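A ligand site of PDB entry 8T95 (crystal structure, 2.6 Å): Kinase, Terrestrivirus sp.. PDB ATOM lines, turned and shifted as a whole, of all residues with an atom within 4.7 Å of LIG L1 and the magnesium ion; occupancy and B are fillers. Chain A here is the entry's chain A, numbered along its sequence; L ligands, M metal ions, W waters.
N3 of LIG L1 is in hydrogen-bond range of O of Glu 97, 2.7 Å away. The backbone NH (N) of Ser 43 sits close to an oxygen (O2) of LIG L1 (3.0 Å). OG of Ser 43 lies within hydrogen-bond range of O2 of LIG L1 (2.7 Å). O9 of LIG L1 is in hydrogen-bond range of OD2 of Asp 110 (2.8 Å). The side-chain amino group of Lys 56 is in salt-bridge range of an oxygen (O5) of LIG L1 (2.9 Å). The backbone NH of Leu 99 is in hydrogen-bond range of a nitrogen (N4) of LIG L1. The backbone NH (N) of Ile 39 lies within hydrogen-bond range of an oxygen (O10) of LIG L1, 3.0 Å away. The backbone NH (N) of Arg 42 is in hydrogen-bond range of an oxygen (O2) of LIG L1, at 3.2 Å. O9 of LIG L1 lies within hydrogen-bond range of N of Ala 40 (3.2 Å). The backbone NH (N) of Gly 41 lies close to an oxygen (O8) of LG2 L2 (3.4 Å). The guanidinium group of Arg 42 is in salt-bridge range of an oxygen (O1) of LG2 L2. The side-chain amino group (NZ) of Lys 112 lies within salt-bridge range of an oxygen (O12) of LG2 L2, at 3.3 Å.
The side-chain carboxylate of Asp 215 lies within salt-bridge range of the side-chain amino group of Lys 56 (3.5 Å). The guanidinium group of Arg 38 lies close to the backbone carbonyl oxygen of Ser 43, at 3.2 Å. The side-chain carboxylate (OD1) of Asp 110 lies within hydrogen-bond range of the side-chain hydroxyl (OG) of Ser 197 (2.8 Å). NH2 of Arg 38 lies within hydrogen-bond range of O of Gly 41, at 2.7 Å. O of Ile 54 sits at hydrogen-bond distance from N of Leu 96. The backbone NH (N) of Phe 36 sits at hydrogen-bond distance from the backbone carbonyl oxygen (O) of Ile 45 (3.2 Å). The side-chain hydroxyl (OG1) of Thr 100 sits at hydrogen-bond distance from the side-chain carboxylate (OD1) of Asp 98 (2.7 Å).
Phe 36 touches LIG L1. Arg 38 touches LIG L1 (C to O10, 3.9 Å). Gly 41 touches LIG L1. Ile 45 touches LIG L1. CD1 of Ile 54 touches C8 of LIG L1, at 3.3 Å. Pro 84 touches LIG L1. Asp 98 touches LIG L1 (OD1 to C9, 3.7 Å). CD1 of Ile 199 touches C3 of LIG L1, at 3.9 Å. Hydrophobic or aromatic side chains that line LIG L1: Phe 36, Ile 39, Ala 40, Ile 45, Ile 54, Pro 84, Leu 99 and Ile 199.
Within 4 Å of the magnesium ion: Asp 215. The nearest printed residue that does not touch the magnesium ion is Ser 197 (4.2 Å).
The magnesium ion is bound by O1 of LIG L1, OD2 of Asp 215, water W2, O4 of LIG L1, O7 of LG2 L2 and water W4. The magnesium ion has six donor atoms within binding distance.
Water W2 bridges the side-chain hydroxyl of Ser 197 (2.5 Å) and the backbone carbonyl oxygen of Gly 195 (2.8 Å). Water W4 lies within hydrogen-bond range of OD2 of Asp 110 (2.6 Å) and O9 of LG2 L2 (3.2 Å).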
ATOM      1  N   PHE A  36      21.887  26.910  31.532  1.00  0.00           N
ATOM      2  CA  PHE A  36      21.192  27.842  30.620  1.00  0.00           C
ATOM      3  C   PHE A  36      20.596  28.991  31.434  1.00  0.00           C
ATOM      4  O   PHE A  36      19.936  28.759  32.448  1.00  0.00           O
ATOM      5  CB  PHE A  36      20.125  27.112  29.797  1.00  0.00           C
ATOM      6  CG  PHE A  36      19.573  27.953  28.667  1.00  0.00           C
ATOM      7  CD1 PHE A  36      20.297  28.111  27.479  1.00  0.00           C
ATOM      8  CD2 PHE A  36      18.385  28.651  28.806  1.00  0.00           C
ATOM      9  CE1 PHE A  36      19.813  28.911  26.455  1.00  0.00           C
ATOM     10  CE2 PHE A  36      17.904  29.465  27.786  1.00  0.00           C
ATOM     11  CZ  PHE A  36      18.614  29.585  26.610  1.00  0.00           C
ATOM     12  N   PRO A  37      20.793  30.270  31.007  1.00  0.00           N
ATOM     13  CA  PRO A  37      20.188  31.422  31.682  1.00  0.00           C
ATOM     14  C   PRO A  37      18.667  31.531  31.494  1.00  0.00           C
ATOM     15  O   PRO A  37      18.212  32.285  30.646  1.00  0.00           O
ATOM     16  CB  PRO A  37      20.902  32.645  31.057  1.00  0.00           C
ATOM     17  CG  PRO A  37      21.323  32.149  29.677  1.00  0.00           C
ATOM     18  CD  PRO A  37      21.629  30.667  29.856  1.00  0.00           C
ATOM     19  N   ARG A  38      17.908  30.775  32.283  1.00  0.00           N
ATOM     20  CA  ARG A  38      16.432  30.834  32.328  1.00  0.00           C
ATOM     21  C   ARG A  38      15.953  32.258  32.663  1.00  0.00           C
ATOM     22  O   ARG A  38      16.664  32.987  33.357  1.00  0.00           O
ATOM     23  CB  ARG A  38      15.870  29.847  33.354  1.00  0.00           C
ATOM     24  CG  ARG A  38      15.830  28.418  32.844  1.00  0.00           C
ATOM     25  CD  ARG A  38      16.105  27.449  33.963  1.00  0.00           C
ATOM     26  NE  ARG A  38      15.158  27.642  35.041  1.00  0.00           N
ATOM     27  CZ  ARG A  38      15.375  27.319  36.329  1.00  0.00           C
ATOM     28  NH1 ARG A  38      16.523  26.783  36.710  1.00  0.00           N
ATOM     29  NH2 ARG A  38      14.422  27.529  37.211  1.00  0.00           N
ATOM     30  N   ILE A  39      14.793  32.629  32.161  1.00  0.00           N
ATOM     31  CA  ILE A  39      14.092  33.880  32.557  1.00  0.00           C
ATOM     32  C   ILE A  39      13.080  33.519  33.635  1.00  0.00           C
ATOM     33  O   ILE A  39      12.859  34.354  34.495  1.00  0.00           O
ATOM     34  CB  ILE A  39      13.486  34.596  31.321  1.00  0.00           C
ATOM     35  CG1 ILE A  39      14.528  35.484  30.659  1.00  0.00           C
ATOM     36  CG2 ILE A  39      12.262  35.399  31.695  1.00  0.00           C
ATOM     37  CD1 ILE A  39      15.219  36.437  31.608  1.00  0.00           C
ATOM     38  N   ALA A  40      12.527  32.310  33.618  1.00  0.00           N
ATOM     39  CA  ALA A  40      11.558  31.847  34.637  1.00  0.00           C
ATOM     40  C   ALA A  40      11.497  30.321  34.602  1.00  0.00           C
ATOM     41  O   ALA A  40      12.392  29.702  34.003  1.00  0.00           O
ATOM     42  CB  ALA A  40      10.208  32.482  34.373  1.00  0.00           C
ATOM     43  N   GLY A  41      10.497  29.731  35.234  1.00  0.00           N
ATOM     44  CA  GLY A  41      10.424  28.264  35.404  1.00  0.00           C
ATOM     45  C   GLY A  41      11.197  27.842  36.630  1.00  0.00           C
ATOM     46  O   GLY A  41      11.947  28.685  37.182  1.00  0.00           O
ATOM     47  N   ARG A  42      10.998  26.592  37.057  1.00  0.00           N
ATOM     48  CA  ARG A  42      11.762  25.922  38.137  1.00  0.00           C
ATOM     49  C   ARG A  42      12.569  24.744  37.543  1.00  0.00           C
ATOM     50  O   ARG A  42      13.316  24.104  38.306  1.00  0.00           O
ATOM     51  CB  ARG A  42      10.797  25.507  39.247  1.00  0.00           C
ATOM     52  CG  ARG A  42      10.301  26.652  40.122  1.00  0.00           C
ATOM     53  CD  ARG A  42       8.986  27.256  39.628  1.00  0.00           C
ATOM     54  NE  ARG A  42       8.422  28.333  40.437  1.00  0.00           N
ATOM     55  CZ  ARG A  42       7.587  28.201  41.465  1.00  0.00           C
ATOM     56  NH1 ARG A  42       7.190  27.003  41.880  1.00  0.00           N
ATOM     57  NH2 ARG A  42       7.128  29.274  42.089  1.00  0.00           N
ATOM     58  N   SER A  43      12.464  24.524  36.213  1.00  0.00           N
ATOM     59  CA  SER A  43      12.959  23.333  35.483  1.00  0.00           C
ATOM     60  C   SER A  43      14.487  23.346  35.327  1.00  0.00           C
ATOM     61  O   SER A  43      15.108  24.421  35.168  1.00  0.00           O
ATOM     62  CB  SER A  43      12.306  23.192  34.121  1.00  0.00           C
ATOM     63  OG  SER A  43      10.945  22.787  34.245  1.00  0.00           O
ATOM     64  N   ILE A  45      17.394  23.102  33.061  1.00  0.00           N
ATOM     65  CA  ILE A  45      17.699  23.384  31.622  1.00  0.00           C
ATOM     66  C   ILE A  45      19.187  23.698  31.507  1.00  0.00           C
ATOM     67  O   ILE A  45      19.644  24.699  32.102  1.00  0.00           O
ATOM     68  CB  ILE A  45      16.859  24.554  31.072  1.00  0.00           C
ATOM     69  CG1 ILE A  45      15.356  24.299  31.199  1.00  0.00           C
ATOM     70  CG2 ILE A  45      17.267  24.857  29.629  1.00  0.00           C
ATOM     71  CD1 ILE A  45      14.482  25.468  30.805  1.00  0.00           C
ATOM     72  N   ILE A  54      19.266  23.182  23.652  1.00  0.00           N
ATOM     73  CA  ILE A  54      19.130  23.173  25.128  1.00  0.00           C
ATOM     74  C   ILE A  54      18.486  21.840  25.511  1.00  0.00           C
ATOM     75  O   ILE A  54      17.689  21.293  24.718  1.00  0.00           O
ATOM     76  CB  ILE A  54      18.325  24.376  25.626  1.00  0.00           C
ATOM     77  CG1 ILE A  54      16.962  24.483  24.942  1.00  0.00           C
ATOM     78  CG2 ILE A  54      19.136  25.640  25.446  1.00  0.00           C
ATOM     79  CD1 ILE A  54      15.983  25.349  25.694  1.00  0.00           C
ATOM     80  N   LYS A  56      16.189  20.244  28.370  1.00  0.00           N
ATOM     81  CA  LYS A  56      15.191  20.497  29.423  1.00  0.00           C
ATOM     82  C   LYS A  56      14.844  19.148  30.034  1.00  0.00           C
ATOM     83  O   LYS A  56      14.497  18.257  29.270  1.00  0.00           O
ATOM     84  CB  LYS A  56      13.960  21.222  28.866  1.00  0.00           C
ATOM     85  CG  LYS A  56      12.747  21.160  29.790  1.00  0.00           C
ATOM     86  CD  LYS A  56      11.618  22.066  29.404  1.00  0.00           C
ATOM     87  CE  LYS A  56      10.509  21.973  30.431  1.00  0.00           C
ATOM     88  NZ  LYS A  56       9.284  22.660  29.956  1.00  0.00           N
ATOM     89  N   PRO A  84       9.377  25.739  19.243  1.00  0.00           N
ATOM     90  CA  PRO A  84      10.750  25.345  18.989  1.00  0.00           C
ATOM     91  C   PRO A  84      10.769  23.864  18.606  1.00  0.00           C
ATOM     92  O   PRO A  84       9.996  23.105  19.199  1.00  0.00           O
ATOM     93  CB  PRO A  84      11.424  25.511  20.355  1.00  0.00           C
ATOM     94  CG  PRO A  84      10.285  25.426  21.342  1.00  0.00           C
ATOM     95  CD  PRO A  84       9.167  26.144  20.635  1.00  0.00           C
ATOM     96  N   LEU A  96      15.858  20.508  22.642  1.00  0.00           N
ATOM     97  CA  LEU A  96      15.008  21.590  22.093  1.00  0.00           C
ATOM     98  C   LEU A  96      15.859  22.616  21.344  1.00  0.00           C
ATOM     99  O   LEU A  96      16.983  22.909  21.776  1.00  0.00           O
ATOM    100  CB  LEU A  96      14.270  22.274  23.252  1.00  0.00           C
ATOM    101  CG  LEU A  96      13.181  21.439  23.911  1.00  0.00           C
ATOM    102  CD1 LEU A  96      12.540  22.215  25.056  1.00  0.00           C
ATOM    103  CD2 LEU A  96      12.126  21.008  22.909  1.00  0.00           C
ATOM    104  N   GLU A  97      15.300  23.177  20.290  1.00  0.00           N
ATOM    105  CA  GLU A  97      15.905  24.350  19.620  1.00  0.00           C
ATOM    106  C   GLU A  97      16.072  25.461  20.669  1.00  0.00           C
ATOM    107  O   GLU A  97      15.116  25.724  21.413  1.00  0.00           O
ATOM    108  CB  GLU A  97      15.038  24.727  18.426  1.00  0.00           C
ATOM    109  CG  GLU A  97      15.393  26.053  17.811  1.00  0.00           C
ATOM    110  CD  GLU A  97      14.336  26.607  16.878  1.00  0.00           C
ATOM    111  OE1 GLU A  97      13.297  25.931  16.654  1.00  0.00           O
ATOM    112  OE2 GLU A  97      14.534  27.747  16.417  1.00  0.00           O
ATOM    113  N   ASP A  98      17.274  26.002  20.771  1.00  0.00           N
ATOM    114  CA  ASP A  98      17.581  27.172  21.625  1.00  0.00           C
ATOM    115  C   ASP A  98      17.145  28.424  20.876  1.00  0.00           C
ATOM    116  O   ASP A  98      17.810  28.793  19.903  1.00  0.00           O
ATOM    117  CB  ASP A  98      19.067  27.204  21.973  1.00  0.00           C
ATOM    118  CG  ASP A  98      19.523  28.461  22.714  1.00  0.00           C
ATOM    119  OD1 ASP A  98      18.650  29.207  23.137  1.00  0.00           O
ATOM    120  OD2 ASP A  98      20.742  28.675  22.831  1.00  0.00           O
ATOM    121  N   LEU A  99      16.069  29.063  21.325  1.00  0.00           N
ATOM    122  CA  LEU A  99      15.425  30.224  20.659  1.00  0.00           C
ATOM    123  C   LEU A  99      16.306  31.456  20.739  1.00  0.00           C
ATOM    124  O   LEU A  99      16.023  32.398  20.023  1.00  0.00           O
ATOM    125  CB  LEU A  99      14.076  30.475  21.336  1.00  0.00           C
ATOM    126  CG  LEU A  99      13.067  29.346  21.148  1.00  0.00           C
ATOM    127  CD1 LEU A  99      11.864  29.547  22.028  1.00  0.00           C
ATOM    128  CD2 LEU A  99      12.659  29.253  19.676  1.00  0.00           C
ATOM    129  N   THR A 100      17.320  31.473  21.597  1.00  0.00           N
ATOM    130  CA  THR A 100      18.218  32.658  21.759  1.00  0.00           C
ATOM    131  C   THR A 100      19.441  32.513  20.853  1.00  0.00           C
ATOM    132  O   THR A 100      20.186  33.481  20.789  1.00  0.00           O
ATOM    133  CB  THR A 100      18.664  32.818  23.206  1.00  0.00           C
ATOM    134  OG1 THR A 100      19.555  31.723  23.452  1.00  0.00           O
ATOM    135  CG2 THR A 100      17.507  32.809  24.172  1.00  0.00           C
ATOM    136  N   VAL A 108      14.856  38.557  26.340  1.00  0.00           N
ATOM    137  CA  VAL A 108      13.816  37.494  26.469  1.00  0.00           C
ATOM    138  C   VAL A 108      12.792  37.956  27.508  1.00  0.00           C
ATOM    139  O   VAL A 108      13.221  38.384  28.581  1.00  0.00           O
ATOM    140  CB  VAL A 108      14.459  36.162  26.894  1.00  0.00           C
ATOM    141  CG1 VAL A 108      13.442  35.030  26.939  1.00  0.00           C
ATOM    142  CG2 VAL A 108      15.605  35.787  25.979  1.00  0.00           C
ATOM    143  N   ASP A 110       9.272  36.124  29.325  1.00  0.00           N
ATOM    144  CA  ASP A 110       8.392  34.933  29.473  1.00  0.00           C
ATOM    145  C   ASP A 110       7.022  35.436  29.923  1.00  0.00           C
ATOM    146  O   ASP A 110       6.961  36.075  30.965  1.00  0.00           O
ATOM    147  CB  ASP A 110       9.008  33.898  30.405  1.00  0.00           C
ATOM    148  CG  ASP A 110       8.128  32.693  30.683  1.00  0.00           C
ATOM    149  OD1 ASP A 110       6.891  32.871  30.639  1.00  0.00           O
ATOM    150  OD2 ASP A 110       8.662  31.617  30.974  1.00  0.00           O
ATOM    151  N   LYS A 112       3.261  33.894  30.749  1.00  0.00           N
ATOM    152  CA  LYS A 112       2.289  32.779  30.922  1.00  0.00           C
ATOM    153  C   LYS A 112       0.921  33.193  30.366  1.00  0.00           C
ATOM    154  O   LYS A 112       0.316  34.141  30.859  1.00  0.00           O
ATOM    155  CB  LYS A 112       2.224  32.407  32.403  1.00  0.00           C
ATOM    156  CG  LYS A 112       1.378  31.188  32.713  1.00  0.00           C
ATOM    157  CD  LYS A 112       2.131  29.918  32.571  1.00  0.00           C
ATOM    158  CE  LYS A 112       3.172  29.734  33.657  1.00  0.00           C
ATOM    159  NZ  LYS A 112       3.158  28.330  34.126  1.00  0.00           N
ATOM    160  N   GLY A 195      -0.555  26.262  31.445  1.00  0.00           N
ATOM    161  CA  GLY A 195       0.857  26.468  31.826  1.00  0.00           C
ATOM    162  C   GLY A 195       1.723  26.986  30.698  1.00  0.00           C
ATOM    163  O   GLY A 195       2.876  27.304  31.021  1.00  0.00           O
ATOM    164  N   SER A 197       3.707  29.215  27.919  1.00  0.00           N
ATOM    165  CA  SER A 197       4.216  30.602  27.910  1.00  0.00           C
ATOM    166  C   SER A 197       4.519  31.001  26.482  1.00  0.00           C
ATOM    167  O   SER A 197       4.784  30.128  25.652  1.00  0.00           O
ATOM    168  CB  SER A 197       5.437  30.761  28.770  1.00  0.00           C
ATOM    169  OG  SER A 197       5.111  30.717  30.140  1.00  0.00           O
ATOM    170  N   ILE A 199       7.485  33.119  24.717  1.00  0.00           N
ATOM    171  CA  ILE A 199       8.863  33.626  24.863  1.00  0.00           C
ATOM    172  C   ILE A 199       9.047  34.663  23.783  1.00  0.00           C
ATOM    173  O   ILE A 199       9.209  34.262  22.623  1.00  0.00           O
ATOM    174  CB  ILE A 199       9.877  32.486  24.735  1.00  0.00           C
ATOM    175  CG1 ILE A 199       9.532  31.340  25.691  1.00  0.00           C
ATOM    176  CG2 ILE A 199      11.283  33.003  24.961  1.00  0.00           C
ATOM    177  CD1 ILE A 199       9.460  31.764  27.145  1.00  0.00           C
ATOM    178  N   VAL A 214       6.013  27.760  24.315  1.00  0.00           N
ATOM    179  CA  VAL A 214       6.809  26.710  25.024  1.00  0.00           C
ATOM    180  C   VAL A 214       6.035  26.189  26.266  1.00  0.00           C
ATOM    181  O   VAL A 214       5.115  26.890  26.718  1.00  0.00           O
ATOM    182  CB  VAL A 214       8.184  27.253  25.444  1.00  0.00           C
ATOM    183  CG1 VAL A 214       8.897  27.907  24.295  1.00  0.00           C
ATOM    184  CG2 VAL A 214       8.062  28.198  26.627  1.00  0.00           C
ATOM    185  N   ASP A 215       6.482  25.040  26.795  1.00  0.00           N
ATOM    186  CA  ASP A 215       6.096  24.437  28.098  1.00  0.00           C
ATOM    187  C   ASP A 215       4.743  23.732  27.957  1.00  0.00           C
ATOM    188  O   ASP A 215       3.702  24.325  28.335  1.00  0.00           O
ATOM    189  CB  ASP A 215       6.079  25.442  29.243  1.00  0.00           C
ATOM    190  CG  ASP A 215       6.127  24.790  30.617  1.00  0.00           C
ATOM    191  OD1 ASP A 215       5.989  23.521  30.672  1.00  0.00           O
ATOM    192  OD2 ASP A 215       6.322  25.534  31.607  1.00  0.00           O
HETATM  193  P1  LIG L   1       9.330  25.505  33.188  1.00  0.00           P
HETATM  194  O1  LIG L   1       8.410  26.665  33.454  1.00  0.00           O
HETATM  195  O2  LIG L   1      10.463  25.485  34.132  1.00  0.00           O
HETATM  196  O3  LIG L   1       8.563  24.168  33.093  1.00  0.00           O
HETATM  197  P2  LIG L   1       9.653  26.493  30.407  1.00  0.00           P
HETATM  198  O4  LIG L   1       8.561  27.497  30.644  1.00  0.00           O
HETATM  199  O5  LIG L   1       9.509  25.485  29.321  1.00  0.00           O
HETATM  200  O6  LIG L   1      10.028  25.670  31.743  1.00  0.00           O
HETATM  201  O7  LIG L   1      11.031  27.298  30.250  1.00  0.00           O
HETATM  202  C1  LIG L   1      11.333  28.252  31.299  1.00  0.00           C
HETATM  203  C2  LIG L   1      12.342  29.241  30.777  1.00  0.00           C
HETATM  204  O8  LIG L   1      13.301  28.559  29.933  1.00  0.00           O
HETATM  205  C3  LIG L   1      11.771  30.382  29.921  1.00  0.00           C
HETATM  206  O9  LIG L   1      11.404  31.460  30.769  1.00  0.00           O
HETATM  207  C4  LIG L   1      12.932  30.698  28.970  1.00  0.00           C
HETATM  208  O10 LIG L   1      13.847  31.614  29.505  1.00  0.00           O
HETATM  209  C5  LIG L   1      13.625  29.347  28.808  1.00  0.00           C
HETATM  210  N1  LIG L   1      13.297  28.562  27.619  1.00  0.00           N
HETATM  211  C6  LIG L   1      12.441  27.489  27.510  1.00  0.00           C
HETATM  212  N2  LIG L   1      12.458  26.910  26.329  1.00  0.00           N
HETATM  213  C7  LIG L   1      13.399  27.628  25.619  1.00  0.00           C
HETATM  214  C8  LIG L   1      13.895  27.510  24.303  1.00  0.00           C
HETATM  215  N3  LIG L   1      13.534  26.551  23.446  1.00  0.00           N
HETATM  216  N4  LIG L   1      14.867  28.356  23.920  1.00  0.00           N
HETATM  217  C9  LIG L   1      15.292  29.294  24.790  1.00  0.00           C
HETATM  218  N5  LIG L   1      14.886  29.527  26.036  1.00  0.00           N
HETATM  219  C10 LIG L   1      13.934  28.640  26.395  1.00  0.00           C
HETATM  220  O1  LG2 L   2       8.919  23.994  40.974  1.00  0.00           O
HETATM  221  P1  LG2 L   2       7.592  23.552  40.533  1.00  0.00           P
HETATM  222  O2  LG2 L   2       7.615  22.414  39.412  1.00  0.00           O
HETATM  223  O3  LG2 L   2       6.570  23.307  41.764  1.00  0.00           O
HETATM  224  O4  LG2 L   2       6.916  24.871  39.851  1.00  0.00           O
HETATM  225  C1  LG2 L   2       5.904  24.937  38.772  1.00  0.00           C
HETATM  226  C2  LG2 L   2       6.324  26.105  37.854  1.00  0.00           C
HETATM  227  O5  LG2 L   2       7.156  25.538  36.832  1.00  0.00           O
HETATM  228  C3  LG2 L   2       5.190  26.900  37.199  1.00  0.00           C
HETATM  229  O6  LG2 L   2       5.600  28.264  36.845  1.00  0.00           O
HETATM  230  P2  LG2 L   2       6.530  28.620  35.593  1.00  0.00           P
HETATM  231  O7  LG2 L   2       5.923  27.923  34.281  1.00  0.00           O
HETATM  232  O8  LG2 L   2       7.719  27.999  36.149  1.00  0.00           O
HETATM  233  O9  LG2 L   2       6.523  30.252  35.550  1.00  0.00           O
HETATM  234  C4  LG2 L   2       4.044  27.125  38.120  1.00  0.00           C
HETATM  235  O10 LG2 L   2       3.078  27.663  37.266  1.00  0.00           O
HETATM  236  P3  LG2 L   2       1.905  28.625  37.629  1.00  0.00           P
HETATM  237  O11 LG2 L   2       2.490  30.106  37.283  1.00  0.00           O
HETATM  238  O12 LG2 L   2       0.865  28.191  36.520  1.00  0.00           O
HETATM  239  O13 LG2 L   2       1.564  28.497  39.067  1.00  0.00           O
HETATM  240  C5  LG2 L   2       3.507  25.838  38.594  1.00  0.00           C
HETATM  241  O14 LG2 L   2       2.362  26.152  39.405  1.00  0.00           O
HETATM  242  C6  LG2 L   2       4.529  25.093  39.433  1.00  0.00           C
HETATM  243  O15 LG2 L   2       4.002  23.780  39.674  1.00  0.00           O
HETATM  244  P4  LG2 L   2       3.189  23.418  41.013  1.00  0.00           P
HETATM  245  O16 LG2 L   2       4.248  23.765  42.183  1.00  0.00           O
HETATM  246  O17 LG2 L   2       2.905  21.863  40.789  1.00  0.00           O
HETATM  247  O18 LG2 L   2       2.015  24.297  41.024  1.00  0.00           O
HETATM  248 MG    MG M   1       6.928  27.521  32.221  1.00  0.00          MG
HETATM  249  O   HOH W   1      10.537  24.420  26.984  1.00  0.00           O
HETATM  250  O   HOH W   2       5.433  28.355  30.751  1.00  0.00           O
HETATM  251  O   HOH W   3      15.458  32.102  27.595  1.00  0.00           O
HETATM  252  O   HOH W   4       7.886  29.761  32.643  1.00  0.00           O
